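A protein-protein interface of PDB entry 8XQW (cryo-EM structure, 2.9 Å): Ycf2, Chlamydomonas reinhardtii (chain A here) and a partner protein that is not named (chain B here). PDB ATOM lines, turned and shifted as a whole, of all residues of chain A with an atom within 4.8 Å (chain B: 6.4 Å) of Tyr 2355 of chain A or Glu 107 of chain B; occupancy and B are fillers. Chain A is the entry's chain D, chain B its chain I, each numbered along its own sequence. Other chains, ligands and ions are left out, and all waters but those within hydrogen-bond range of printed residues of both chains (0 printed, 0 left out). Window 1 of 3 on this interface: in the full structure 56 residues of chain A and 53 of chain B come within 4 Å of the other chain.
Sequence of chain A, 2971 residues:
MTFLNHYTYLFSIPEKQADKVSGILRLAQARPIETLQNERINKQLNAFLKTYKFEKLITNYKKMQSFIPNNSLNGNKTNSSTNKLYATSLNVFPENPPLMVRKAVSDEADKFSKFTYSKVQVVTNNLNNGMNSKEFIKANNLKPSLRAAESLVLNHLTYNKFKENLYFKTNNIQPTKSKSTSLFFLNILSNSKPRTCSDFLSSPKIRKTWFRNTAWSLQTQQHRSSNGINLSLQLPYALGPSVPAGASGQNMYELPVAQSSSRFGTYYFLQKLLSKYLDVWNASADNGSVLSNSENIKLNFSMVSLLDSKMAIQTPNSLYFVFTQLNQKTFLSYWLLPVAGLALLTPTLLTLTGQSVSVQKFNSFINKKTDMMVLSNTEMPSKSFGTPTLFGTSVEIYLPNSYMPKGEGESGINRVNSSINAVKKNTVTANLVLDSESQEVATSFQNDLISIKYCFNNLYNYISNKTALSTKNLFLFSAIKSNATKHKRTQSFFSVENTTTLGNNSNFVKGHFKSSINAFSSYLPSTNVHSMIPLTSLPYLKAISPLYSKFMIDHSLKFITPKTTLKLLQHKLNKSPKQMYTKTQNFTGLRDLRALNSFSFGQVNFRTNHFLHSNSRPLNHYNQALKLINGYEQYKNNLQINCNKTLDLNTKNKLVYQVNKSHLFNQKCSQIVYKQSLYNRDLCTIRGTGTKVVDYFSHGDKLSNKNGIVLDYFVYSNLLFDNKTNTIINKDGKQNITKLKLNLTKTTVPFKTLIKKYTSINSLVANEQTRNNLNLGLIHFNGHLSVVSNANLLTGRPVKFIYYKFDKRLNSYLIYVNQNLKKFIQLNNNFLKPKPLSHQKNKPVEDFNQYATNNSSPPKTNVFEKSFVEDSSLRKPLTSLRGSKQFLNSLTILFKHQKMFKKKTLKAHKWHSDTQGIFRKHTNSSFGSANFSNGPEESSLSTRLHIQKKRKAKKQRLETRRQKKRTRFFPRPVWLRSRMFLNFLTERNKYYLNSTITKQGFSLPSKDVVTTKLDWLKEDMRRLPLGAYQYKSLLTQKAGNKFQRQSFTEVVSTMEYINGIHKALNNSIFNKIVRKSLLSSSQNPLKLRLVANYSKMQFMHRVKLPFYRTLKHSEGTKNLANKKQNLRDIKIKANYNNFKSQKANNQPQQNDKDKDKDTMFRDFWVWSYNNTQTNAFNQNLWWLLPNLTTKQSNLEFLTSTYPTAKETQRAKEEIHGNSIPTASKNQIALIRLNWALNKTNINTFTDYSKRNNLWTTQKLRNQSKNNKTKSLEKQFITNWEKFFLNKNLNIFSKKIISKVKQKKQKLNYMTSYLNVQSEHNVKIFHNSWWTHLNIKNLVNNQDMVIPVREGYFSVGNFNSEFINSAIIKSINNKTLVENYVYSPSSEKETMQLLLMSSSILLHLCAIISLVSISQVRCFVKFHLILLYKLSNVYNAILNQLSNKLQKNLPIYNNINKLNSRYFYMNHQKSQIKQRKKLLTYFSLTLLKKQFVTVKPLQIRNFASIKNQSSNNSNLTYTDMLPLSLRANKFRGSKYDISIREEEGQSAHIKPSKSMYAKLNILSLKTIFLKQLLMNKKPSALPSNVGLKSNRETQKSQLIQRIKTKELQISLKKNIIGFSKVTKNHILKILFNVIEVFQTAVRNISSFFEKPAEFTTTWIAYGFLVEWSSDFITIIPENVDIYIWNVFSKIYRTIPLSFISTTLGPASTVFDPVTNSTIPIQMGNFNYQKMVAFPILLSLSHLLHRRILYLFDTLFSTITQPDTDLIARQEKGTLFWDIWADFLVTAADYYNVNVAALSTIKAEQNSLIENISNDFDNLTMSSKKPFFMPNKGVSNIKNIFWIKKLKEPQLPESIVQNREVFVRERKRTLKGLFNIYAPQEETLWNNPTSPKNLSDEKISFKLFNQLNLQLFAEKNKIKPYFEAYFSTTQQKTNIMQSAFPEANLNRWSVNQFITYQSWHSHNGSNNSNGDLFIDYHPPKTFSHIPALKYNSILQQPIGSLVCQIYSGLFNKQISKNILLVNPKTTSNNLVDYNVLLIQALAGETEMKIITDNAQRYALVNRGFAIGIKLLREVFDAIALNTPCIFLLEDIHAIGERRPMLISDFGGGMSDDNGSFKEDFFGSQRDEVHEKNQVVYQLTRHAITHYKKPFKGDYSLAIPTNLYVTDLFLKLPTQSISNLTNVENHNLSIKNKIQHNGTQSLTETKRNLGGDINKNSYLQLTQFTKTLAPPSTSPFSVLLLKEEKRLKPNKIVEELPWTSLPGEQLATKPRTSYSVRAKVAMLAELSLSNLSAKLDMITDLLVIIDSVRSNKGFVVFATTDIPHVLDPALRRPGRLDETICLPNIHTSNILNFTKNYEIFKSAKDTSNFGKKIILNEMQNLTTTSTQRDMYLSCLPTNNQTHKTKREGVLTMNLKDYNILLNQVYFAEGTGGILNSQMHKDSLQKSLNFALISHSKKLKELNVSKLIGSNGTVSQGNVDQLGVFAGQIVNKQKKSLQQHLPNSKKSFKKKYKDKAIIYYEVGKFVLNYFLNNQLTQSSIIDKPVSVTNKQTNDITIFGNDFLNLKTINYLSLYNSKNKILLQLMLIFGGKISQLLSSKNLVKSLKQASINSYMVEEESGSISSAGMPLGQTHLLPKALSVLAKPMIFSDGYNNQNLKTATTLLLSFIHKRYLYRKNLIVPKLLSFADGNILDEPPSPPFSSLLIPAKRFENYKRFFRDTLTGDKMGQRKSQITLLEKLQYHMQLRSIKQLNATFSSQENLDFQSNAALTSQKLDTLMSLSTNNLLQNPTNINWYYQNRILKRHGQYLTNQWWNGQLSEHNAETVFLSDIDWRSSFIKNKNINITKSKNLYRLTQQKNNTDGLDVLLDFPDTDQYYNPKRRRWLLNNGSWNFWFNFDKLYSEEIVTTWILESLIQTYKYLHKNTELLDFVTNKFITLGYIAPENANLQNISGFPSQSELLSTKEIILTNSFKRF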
ATOM      1  N   PHE A2351      -4.126 -13.554 -10.988  1.00  0.00           N
ATOM      2  CA  PHE A2351      -3.029 -13.295 -10.071  1.00  0.00           C
ATOM      3  C   PHE A2351      -2.603 -11.840 -10.121  1.00  0.00           C
ATOM      4  O   PHE A2351      -2.433 -11.209  -9.073  1.00  0.00           O
ATOM      5  CB  PHE A2351      -1.837 -14.187 -10.371  1.00  0.00           C
ATOM      6  CG  PHE A2351      -0.689 -13.964  -9.436  1.00  0.00           C
ATOM      7  CD1 PHE A2351      -0.920 -13.636  -8.112  1.00  0.00           C
ATOM      8  CD2 PHE A2351       0.611 -14.065  -9.873  1.00  0.00           C
ATOM      9  CE1 PHE A2351       0.117 -13.416  -7.247  1.00  0.00           C
ATOM     10  CE2 PHE A2351       1.654 -13.849  -9.006  1.00  0.00           C
ATOM     11  CZ  PHE A2351       1.405 -13.525  -7.691  1.00  0.00           C
ATOM     12  N   THR A2352      -2.397 -11.291 -11.315  1.00  0.00           N
ATOM     13  CA  THR A2352      -1.970  -9.901 -11.387  1.00  0.00           C
ATOM     14  C   THR A2352      -3.021  -8.979 -10.796  1.00  0.00           C
ATOM     15  O   THR A2352      -2.688  -8.016 -10.112  1.00  0.00           O
ATOM     16  CB  THR A2352      -1.656  -9.507 -12.823  1.00  0.00           C
ATOM     17  OG1 THR A2352      -2.785  -9.778 -13.648  1.00  0.00           O
ATOM     18  CG2 THR A2352      -0.479 -10.287 -13.334  1.00  0.00           C
ATOM     19  N   LYS A2353      -4.294  -9.280 -11.006  1.00  0.00           N
ATOM     20  CA  LYS A2353      -5.356  -8.472 -10.436  1.00  0.00           C
ATOM     21  C   LYS A2353      -5.291  -8.463  -8.917  1.00  0.00           C
ATOM     22  O   LYS A2353      -5.294  -7.398  -8.289  1.00  0.00           O
ATOM     23  CB  LYS A2353      -6.692  -9.016 -10.922  1.00  0.00           C
ATOM     24  CG  LYS A2353      -7.895  -8.471 -10.234  1.00  0.00           C
ATOM     25  CD  LYS A2353      -9.122  -9.189 -10.731  1.00  0.00           C
ATOM     26  CE  LYS A2353      -9.606 -10.199  -9.727  1.00  0.00           C
ATOM     27  NZ  LYS A2353     -10.402  -9.524  -8.676  1.00  0.00           N
ATOM     28  N   ASN A2354      -5.232  -9.645  -8.307  1.00  0.00           N
ATOM     29  CA  ASN A2354      -5.205  -9.709  -6.853  1.00  0.00           C
ATOM     30  C   ASN A2354      -3.969  -9.028  -6.293  1.00  0.00           C
ATOM     31  O   ASN A2354      -4.047  -8.289  -5.304  1.00  0.00           O
ATOM     32  CB  ASN A2354      -5.281 -11.159  -6.399  1.00  0.00           C
ATOM     33  CG  ASN A2354      -6.620 -11.777  -6.687  1.00  0.00           C
ATOM     34  OD1 ASN A2354      -7.555 -11.086  -7.064  1.00  0.00           O
ATOM     35  ND2 ASN A2354      -6.725 -13.080  -6.512  1.00  0.00           N
ATOM     36  N   TYR A2355      -2.826  -9.225  -6.933  1.00  0.00           N
ATOM     37  CA  TYR A2355      -1.598  -8.616  -6.448  1.00  0.00           C
ATOM     38  C   TYR A2355      -1.646  -7.098  -6.545  1.00  0.00           C
ATOM     39  O   TYR A2355      -1.264  -6.403  -5.600  1.00  0.00           O
ATOM     40  CB  TYR A2355      -0.424  -9.174  -7.235  1.00  0.00           C
ATOM     41  CG  TYR A2355       0.911  -8.615  -6.864  1.00  0.00           C
ATOM     42  CD1 TYR A2355       1.600  -9.092  -5.774  1.00  0.00           C
ATOM     43  CD2 TYR A2355       1.500  -7.633  -7.630  1.00  0.00           C
ATOM     44  CE1 TYR A2355       2.827  -8.592  -5.442  1.00  0.00           C
ATOM     45  CE2 TYR A2355       2.725  -7.127  -7.306  1.00  0.00           C
ATOM     46  CZ  TYR A2355       3.387  -7.615  -6.215  1.00  0.00           C
ATOM     47  OH  TYR A2355       4.618  -7.110  -5.888  1.00  0.00           O
ATOM     48  N   GLU A2356      -2.101  -6.560  -7.676  1.00  0.00           N
ATOM     49  CA  GLU A2356      -2.151  -5.111  -7.818  1.00  0.00           C
ATOM     50  C   GLU A2356      -3.096  -4.491  -6.810  1.00  0.00           C
ATOM     51  O   GLU A2356      -2.782  -3.450  -6.227  1.00  0.00           O
ATOM     52  CB  GLU A2356      -2.581  -4.717  -9.225  1.00  0.00           C
ATOM     53  CG  GLU A2356      -1.749  -5.298 -10.330  1.00  0.00           C
ATOM     54  CD  GLU A2356      -0.715  -4.355 -10.850  1.00  0.00           C
ATOM     55  OE1 GLU A2356      -0.609  -3.240 -10.312  1.00  0.00           O
ATOM     56  OE2 GLU A2356      -0.003  -4.731 -11.803  1.00  0.00           O
ATOM     57  N   ILE A2357      -4.255  -5.102  -6.582  1.00  0.00           N
ATOM     58  CA  ILE A2357      -5.175  -4.521  -5.612  1.00  0.00           C
ATOM     59  C   ILE A2357      -4.567  -4.541  -4.217  1.00  0.00           C
ATOM     60  O   ILE A2357      -4.590  -3.532  -3.495  1.00  0.00           O
ATOM     61  CB  ILE A2357      -6.521  -5.252  -5.647  1.00  0.00           C
ATOM     62  CG1 ILE A2357      -7.259  -4.934  -6.934  1.00  0.00           C
ATOM     63  CG2 ILE A2357      -7.356  -4.828  -4.488  1.00  0.00           C
ATOM     64  CD1 ILE A2357      -8.590  -5.589  -7.023  1.00  0.00           C
ATOM     65  N   PHE A2358      -3.995  -5.675  -3.819  1.00  0.00           N
ATOM     66  CA  PHE A2358      -3.417  -5.745  -2.486  1.00  0.00           C
ATOM     67  C   PHE A2358      -2.310  -4.719  -2.305  1.00  0.00           C
ATOM     68  O   PHE A2358      -2.225  -4.076  -1.258  1.00  0.00           O
ATOM     69  CB  PHE A2358      -2.893  -7.145  -2.216  1.00  0.00           C
ATOM     70  CG  PHE A2358      -2.494  -7.363  -0.802  1.00  0.00           C
ATOM     71  CD1 PHE A2358      -3.433  -7.662   0.148  1.00  0.00           C
ATOM     72  CD2 PHE A2358      -1.182  -7.261  -0.422  1.00  0.00           C
ATOM     73  CE1 PHE A2358      -3.071  -7.857   1.442  1.00  0.00           C
ATOM     74  CE2 PHE A2358      -0.820  -7.457   0.878  1.00  0.00           C
ATOM     75  CZ  PHE A2358      -1.767  -7.757   1.805  1.00  0.00           C
ATOM     76  N   LYS A2359      -1.454  -4.542  -3.308  1.00  0.00           N
ATOM     77  CA  LYS A2359      -0.384  -3.563  -3.161  1.00  0.00           C
ATOM     78  C   LYS A2359      -0.911  -2.138  -3.154  1.00  0.00           C
ATOM     79  O   LYS A2359      -0.328  -1.273  -2.501  1.00  0.00           O
ATOM     80  CB  LYS A2359       0.649  -3.713  -4.270  1.00  0.00           C
ATOM     81  CG  LYS A2359       1.292  -5.054  -4.322  1.00  0.00           C
ATOM     82  CD  LYS A2359       1.687  -5.524  -2.956  1.00  0.00           C
ATOM     83  CE  LYS A2359       3.023  -4.958  -2.561  1.00  0.00           C
ATOM     84  NZ  LYS A2359       3.443  -5.459  -1.225  1.00  0.00           N
ATOM     85  N   MET A2410       4.308 -14.657   4.687  1.00  0.00           N
ATOM     86  CA  MET A2410       3.525 -15.524   3.830  1.00  0.00           C
ATOM     87  C   MET A2410       3.588 -15.004   2.410  1.00  0.00           C
ATOM     88  O   MET A2410       3.569 -13.796   2.179  1.00  0.00           O
ATOM     89  CB  MET A2410       2.074 -15.578   4.299  1.00  0.00           C
ATOM     90  CG  MET A2410       1.819 -16.553   5.424  1.00  0.00           C
ATOM     91  SD  MET A2410       1.621 -18.228   4.803  1.00  0.00           S
ATOM     92  CE  MET A2410       3.182 -18.950   5.285  1.00  0.00           C
ATOM     93  N   ASN A2411       3.664 -15.915   1.456  1.00  0.00           N
ATOM     94  CA  ASN A2411       3.664 -15.518   0.063  1.00  0.00           C
ATOM     95  C   ASN A2411       2.228 -15.333  -0.396  1.00  0.00           C
ATOM     96  O   ASN A2411       1.375 -16.180  -0.136  1.00  0.00           O
ATOM     97  CB  ASN A2411       4.376 -16.561  -0.785  1.00  0.00           C
ATOM     98  CG  ASN A2411       4.761 -16.039  -2.139  1.00  0.00           C
ATOM     99  OD1 ASN A2411       4.012 -15.299  -2.759  1.00  0.00           O
ATOM    100  ND2 ASN A2411       5.936 -16.417  -2.607  1.00  0.00           N
ATOM    101  N   LEU A2412       1.955 -14.217  -1.067  1.00  0.00           N
ATOM    102  CA  LEU A2412       0.596 -13.937  -1.502  1.00  0.00           C
ATOM    103  C   LEU A2412       0.127 -14.902  -2.571  1.00  0.00           C
ATOM    104  O   LEU A2412      -1.083 -15.129  -2.707  1.00  0.00           O
ATOM    105  CB  LEU A2412       0.497 -12.509  -2.019  1.00  0.00           C
ATOM    106  CG  LEU A2412       0.790 -11.421  -0.993  1.00  0.00           C
ATOM    107  CD1 LEU A2412       0.658 -10.061  -1.628  1.00  0.00           C
ATOM    108  CD2 LEU A2412      -0.137 -11.542   0.189  1.00  0.00           C
ATOM    109  N   ARG B  99       5.910  -8.950 -17.274  1.00  0.00           N
ATOM    110  CA  ARG B  99       5.202  -8.537 -16.073  1.00  0.00           C
ATOM    111  C   ARG B  99       5.157  -9.662 -15.056  1.00  0.00           C
ATOM    112  O   ARG B  99       5.397  -9.441 -13.864  1.00  0.00           O
ATOM    113  CB  ARG B  99       3.795  -8.089 -16.437  1.00  0.00           C
ATOM    114  CG  ARG B  99       2.994  -7.585 -15.281  1.00  0.00           C
ATOM    115  CD  ARG B  99       3.151  -6.090 -15.137  1.00  0.00           C
ATOM    116  NE  ARG B  99       4.092  -5.738 -14.081  1.00  0.00           N
ATOM    117  CZ  ARG B  99       3.732  -5.358 -12.863  1.00  0.00           C
ATOM    118  NH1 ARG B  99       2.450  -5.276 -12.548  1.00  0.00           N
ATOM    119  NH2 ARG B  99       4.651  -5.059 -11.961  1.00  0.00           N
ATOM    120  N   ASP B 102       8.566 -10.180 -13.361  1.00  0.00           N
ATOM    121  CA  ASP B 102       8.896  -9.147 -12.384  1.00  0.00           C
ATOM    122  C   ASP B 102       8.059  -9.275 -11.121  1.00  0.00           C
ATOM    123  O   ASP B 102       8.561  -9.037 -10.016  1.00  0.00           O
ATOM    124  CB  ASP B 102       8.734  -7.766 -12.990  1.00  0.00           C
ATOM    125  CG  ASP B 102       9.482  -7.620 -14.283  1.00  0.00           C
ATOM    126  OD1 ASP B 102      10.513  -8.302 -14.437  1.00  0.00           O
ATOM    127  OD2 ASP B 102       9.042  -6.835 -15.150  1.00  0.00           O
ATOM    128  N   ILE B 103       6.790  -9.659 -11.250  1.00  0.00           N
ATOM    129  CA  ILE B 103       5.970  -9.849 -10.058  1.00  0.00           C
ATOM    130  C   ILE B 103       6.538 -10.967  -9.196  1.00  0.00           C
ATOM    131  O   ILE B 103       6.651 -10.834  -7.972  1.00  0.00           O
ATOM    132  CB  ILE B 103       4.514 -10.130 -10.443  1.00  0.00           C
ATOM    133  CG1 ILE B 103       3.782  -8.836 -10.740  1.00  0.00           C
ATOM    134  CG2 ILE B 103       3.819 -10.846  -9.335  1.00  0.00           C
ATOM    135  CD1 ILE B 103       2.442  -9.060 -11.369  1.00  0.00           C
ATOM    136  N   ASN B 104       6.906 -12.086  -9.819  1.00  0.00           N
ATOM    137  CA  ASN B 104       7.457 -13.190  -9.041  1.00  0.00           C
ATOM    138  C   ASN B 104       8.757 -12.800  -8.366  1.00  0.00           C
ATOM    139  O   ASN B 104       8.984 -13.136  -7.199  1.00  0.00           O
ATOM    140  CB  ASN B 104       7.671 -14.402  -9.928  1.00  0.00           C
ATOM    141  CG  ASN B 104       6.405 -15.156 -10.175  1.00  0.00           C
ATOM    142  OD1 ASN B 104       5.379 -14.876  -9.574  1.00  0.00           O
ATOM    143  ND2 ASN B 104       6.466 -16.134 -11.052  1.00  0.00           N
ATOM    144  N   LYS B 105       9.626 -12.096  -9.082  1.00  0.00           N
ATOM    145  CA  LYS B 105      10.886 -11.657  -8.500  1.00  0.00           C
ATOM    146  C   LYS B 105      10.655 -10.800  -7.261  1.00  0.00           C
ATOM    147  O   LYS B 105      11.235 -11.045  -6.191  1.00  0.00           O
ATOM    148  CB  LYS B 105      11.665 -10.890  -9.555  1.00  0.00           C
ATOM    149  CG  LYS B 105      13.101 -10.706  -9.266  1.00  0.00           C
ATOM    150  CD  LYS B 105      13.675  -9.690 -10.200  1.00  0.00           C
ATOM    151  CE  LYS B 105      15.127  -9.448  -9.887  1.00  0.00           C
ATOM    152  NZ  LYS B 105      15.617  -8.196 -10.511  1.00  0.00           N
ATOM    153  N   ALA B 106       9.796  -9.790  -7.384  1.00  0.00           N
ATOM    154  CA  ALA B 106       9.572  -8.877  -6.274  1.00  0.00           C
ATOM    155  C   ALA B 106       8.947  -9.585  -5.082  1.00  0.00           C
ATOM    156  O   ALA B 106       9.304  -9.304  -3.933  1.00  0.00           O
ATOM    157  CB  ALA B 106       8.686  -7.728  -6.726  1.00  0.00           C
ATOM    158  N   GLU B 107       8.011 -10.496  -5.327  1.00  0.00           N
ATOM    159  CA  GLU B 107       7.365 -11.175  -4.214  1.00  0.00           C
ATOM    160  C   GLU B 107       8.328 -12.100  -3.484  1.00  0.00           C
ATOM    161  O   GLU B 107       8.319 -12.165  -2.249  1.00  0.00           O
ATOM    162  CB  GLU B 107       6.155 -11.946  -4.714  1.00  0.00           C
ATOM    163  CG  GLU B 107       5.323 -12.514  -3.608  1.00  0.00           C
ATOM    164  CD  GLU B 107       4.605 -11.448  -2.817  1.00  0.00           C
ATOM    165  OE1 GLU B 107       4.122 -10.488  -3.442  1.00  0.00           O
ATOM    166  OE2 GLU B 107       4.521 -11.565  -1.574  1.00  0.00           O
ATOM    167  N   ARG B 108       9.176 -12.817  -4.221  1.00  0.00           N
ATOM    168  CA  ARG B 108      10.164 -13.660  -3.563  1.00  0.00           C
ATOM    169  C   ARG B 108      11.095 -12.837  -2.696  1.00  0.00           C
ATOM    170  O   ARG B 108      11.454 -13.248  -1.585  1.00  0.00           O
ATOM    171  CB  ARG B 108      10.968 -14.431  -4.593  1.00  0.00           C
ATOM    172  CG  ARG B 108      10.219 -15.518  -5.266  1.00  0.00           C
ATOM    173  CD  ARG B 108      11.101 -16.206  -6.248  1.00  0.00           C
ATOM    174  NE  ARG B 108      10.323 -16.989  -7.189  1.00  0.00           N
ATOM    175  CZ  ARG B 108      10.677 -17.194  -8.446  1.00  0.00           C
ATOM    176  NH1 ARG B 108      11.798 -16.668  -8.911  1.00  0.00           N
ATOM    177  NH2 ARG B 108       9.904 -17.913  -9.237  1.00  0.00           N
ATOM    178  N   GLN B 109      11.493 -11.662  -3.179  1.00  0.00           N
ATOM    179  CA  GLN B 109      12.381 -10.831  -2.377  1.00  0.00           C
ATOM    180  C   GLN B 109      11.710 -10.344  -1.101  1.00  0.00           C
ATOM    181  O   GLN B 109      12.300 -10.409  -0.016  1.00  0.00           O
ATOM    182  CB  GLN B 109      12.847  -9.644  -3.187  1.00  0.00           C
ATOM    183  CG  GLN B 109      13.822  -8.843  -2.440  1.00  0.00           C
ATOM    184  CD  GLN B 109      15.111  -9.561  -2.327  1.00  0.00           C
ATOM    185  OE1 GLN B 109      15.598 -10.103  -3.304  1.00  0.00           O
ATOM    186  NE2 GLN B 109      15.678  -9.587  -1.141  1.00  0.00           N
ATOM    187  N   ARG B 110      10.493  -9.818  -1.213  1.00  0.00           N
ATOM    188  CA  ARG B 110       9.803  -9.325  -0.029  1.00  0.00           C
ATOM    189  C   ARG B 110       9.642 -10.421   1.010  1.00  0.00           C
ATOM    190  O   ARG B 110       9.816 -10.180   2.211  1.00  0.00           O
ATOM    191  CB  ARG B 110       8.448  -8.756  -0.423  1.00  0.00           C
ATOM    192  CG  ARG B 110       7.636  -8.259   0.727  1.00  0.00           C
ATOM    193  CD  ARG B 110       6.178  -8.163   0.364  1.00  0.00           C
ATOM    194  NE  ARG B 110       5.550  -9.471   0.307  1.00  0.00           N
ATOM    195  CZ  ARG B 110       5.237 -10.192   1.374  1.00  0.00           C
ATOM    196  NH1 ARG B 110       5.492  -9.729   2.580  1.00  0.00           N
ATOM    197  NH2 ARG B 110       4.670 -11.374   1.231  1.00  0.00           N
ATOM    198  N   VAL B 111       9.348 -11.643   0.575  1.00  0.00           N
ATOM    199  CA  VAL B 111       9.170 -12.718   1.544  1.00  0.00           C
ATOM    200  C   VAL B 111      10.488 -13.085   2.209  1.00  0.00           C
ATOM    201  O   VAL B 111      10.528 -13.349   3.413  1.00  0.00           O
ATOM    202  CB  VAL B 111       8.518 -13.932   0.881  1.00  0.00           C
ATOM    203  CG1 VAL B 111       8.504 -15.070   1.827  1.00  0.00           C
ATOM    204  CG2 VAL B 111       7.124 -13.593   0.509  1.00  0.00           C
ATOM    205  N   TRP B 112      11.584 -13.122   1.453  1.00  0.00           N
ATOM    206  CA  TRP B 112      12.867 -13.418   2.084  1.00  0.00           C
ATOM    207  C   TRP B 112      13.206 -12.389   3.148  1.00  0.00           C
ATOM    208  O   TRP B 112      13.702 -12.732   4.226  1.00  0.00           O
ATOM    209  CB  TRP B 112      13.970 -13.469   1.048  1.00  0.00           C
ATOM    210  CG  TRP B 112      15.316 -13.712   1.615  1.00  0.00           C
ATOM    211  CD1 TRP B 112      16.353 -12.856   1.617  1.00  0.00           C
ATOM    212  CD2 TRP B 112      15.780 -14.901   2.243  1.00  0.00           C
ATOM    213  NE1 TRP B 112      17.440 -13.428   2.206  1.00  0.00           N
ATOM    214  CE2 TRP B 112      17.110 -14.693   2.595  1.00  0.00           C
ATOM    215  CE3 TRP B 112      15.198 -16.130   2.535  1.00  0.00           C
ATOM    216  CZ2 TRP B 112      17.861 -15.649   3.238  1.00  0.00           C
ATOM    217  CZ3 TRP B 112      15.946 -17.074   3.167  1.00  0.00           C
ATOM    218  CH2 TRP B 112      17.260 -16.836   3.510  1.00  0.00           C
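Ile 103 of chain B touches Phe 2351 of chain A.
Asn 104 of chain B touches Phe 2351 of chain A.
CG2 of Thr 2352 of chain A touches CD1 of Ile 103 of chain B (3.7 Å).
CG1 of Ile 103 of chain B touches CE2 of Tyr 2355 of chain A, 3.98 Å away.
CE1 of Tyr 2355 of chain A touches OE1 of Glu 107 of chain B, 3.0 Å away.
Val 111 of chain B touches Met 2410 of chain A (CG2 to O, 3.9 Å).
OD1 of Asn 2411 of chain A touches CG of Glu 107 of chain B, 3.2 Å away.
Asn 2411 of chain A touches Val 111 of chain B (CA to CG2, 3.98 Å).
Leu 2412 of chain A touches Glu 107 of chain B.
The guanidinium group of Arg 110 of chain B lies within salt-bridge range of the side-chain carboxylate of Glu 107 of chain B, at 2.8 Å.
Hydrophobic or aromatic side chains of chain A that line the printed part of chain B: Phe 2351, Tyr 2355 and Leu 2412.
Of the 12 printed residues of chain B, 6 touch a printed residue of chain A.
Hydrophobic or aromatic side chains of chain B within 4 Å of the printed part of chain A: Ile 103 and Val 111.
Among the printed residues, Asp or Glu carboxylates within 4 Å of a Lys or Arg side-chain nitrogen of the other chain: Glu 2356 of chain A with Arg 99 of chain B.
The guanidinium group of Arg 99 of chain B lies within salt-bridge range of the side-chain carboxylate of Glu 2356 of chain A (2.6 Å).
O of Met 2410 of chain A lies within hydrogen-bond range of NH2 of Arg 110 of chain B.
Of the printed residues of chain B, Thr 2352 of chain A touches Ile 103.
Asn 2354 of chain A touches none of the printed residues of chain B.
Tyr 2355 of chain A touches just these residues of chain B: Ile 103 (3.98 Å) and Glu 107 (3.0 Å).
Asp 102 of chain B touches none of the printed residues of chain A.
Glu 107 of chain B touches three residues of chain A.
Printed residues of chain A within 4 Å of Val 111 of chain B: Met 2410 and Asn 2411.
The nearest residue of chain A that does not touch Glu 107 of chain B is Met 2410 of chain A (4.5 Å).
The nearest printed residue of chain A that does not touch Arg 110 of chain B is Lys 2359 of chain A (4.2 Å).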
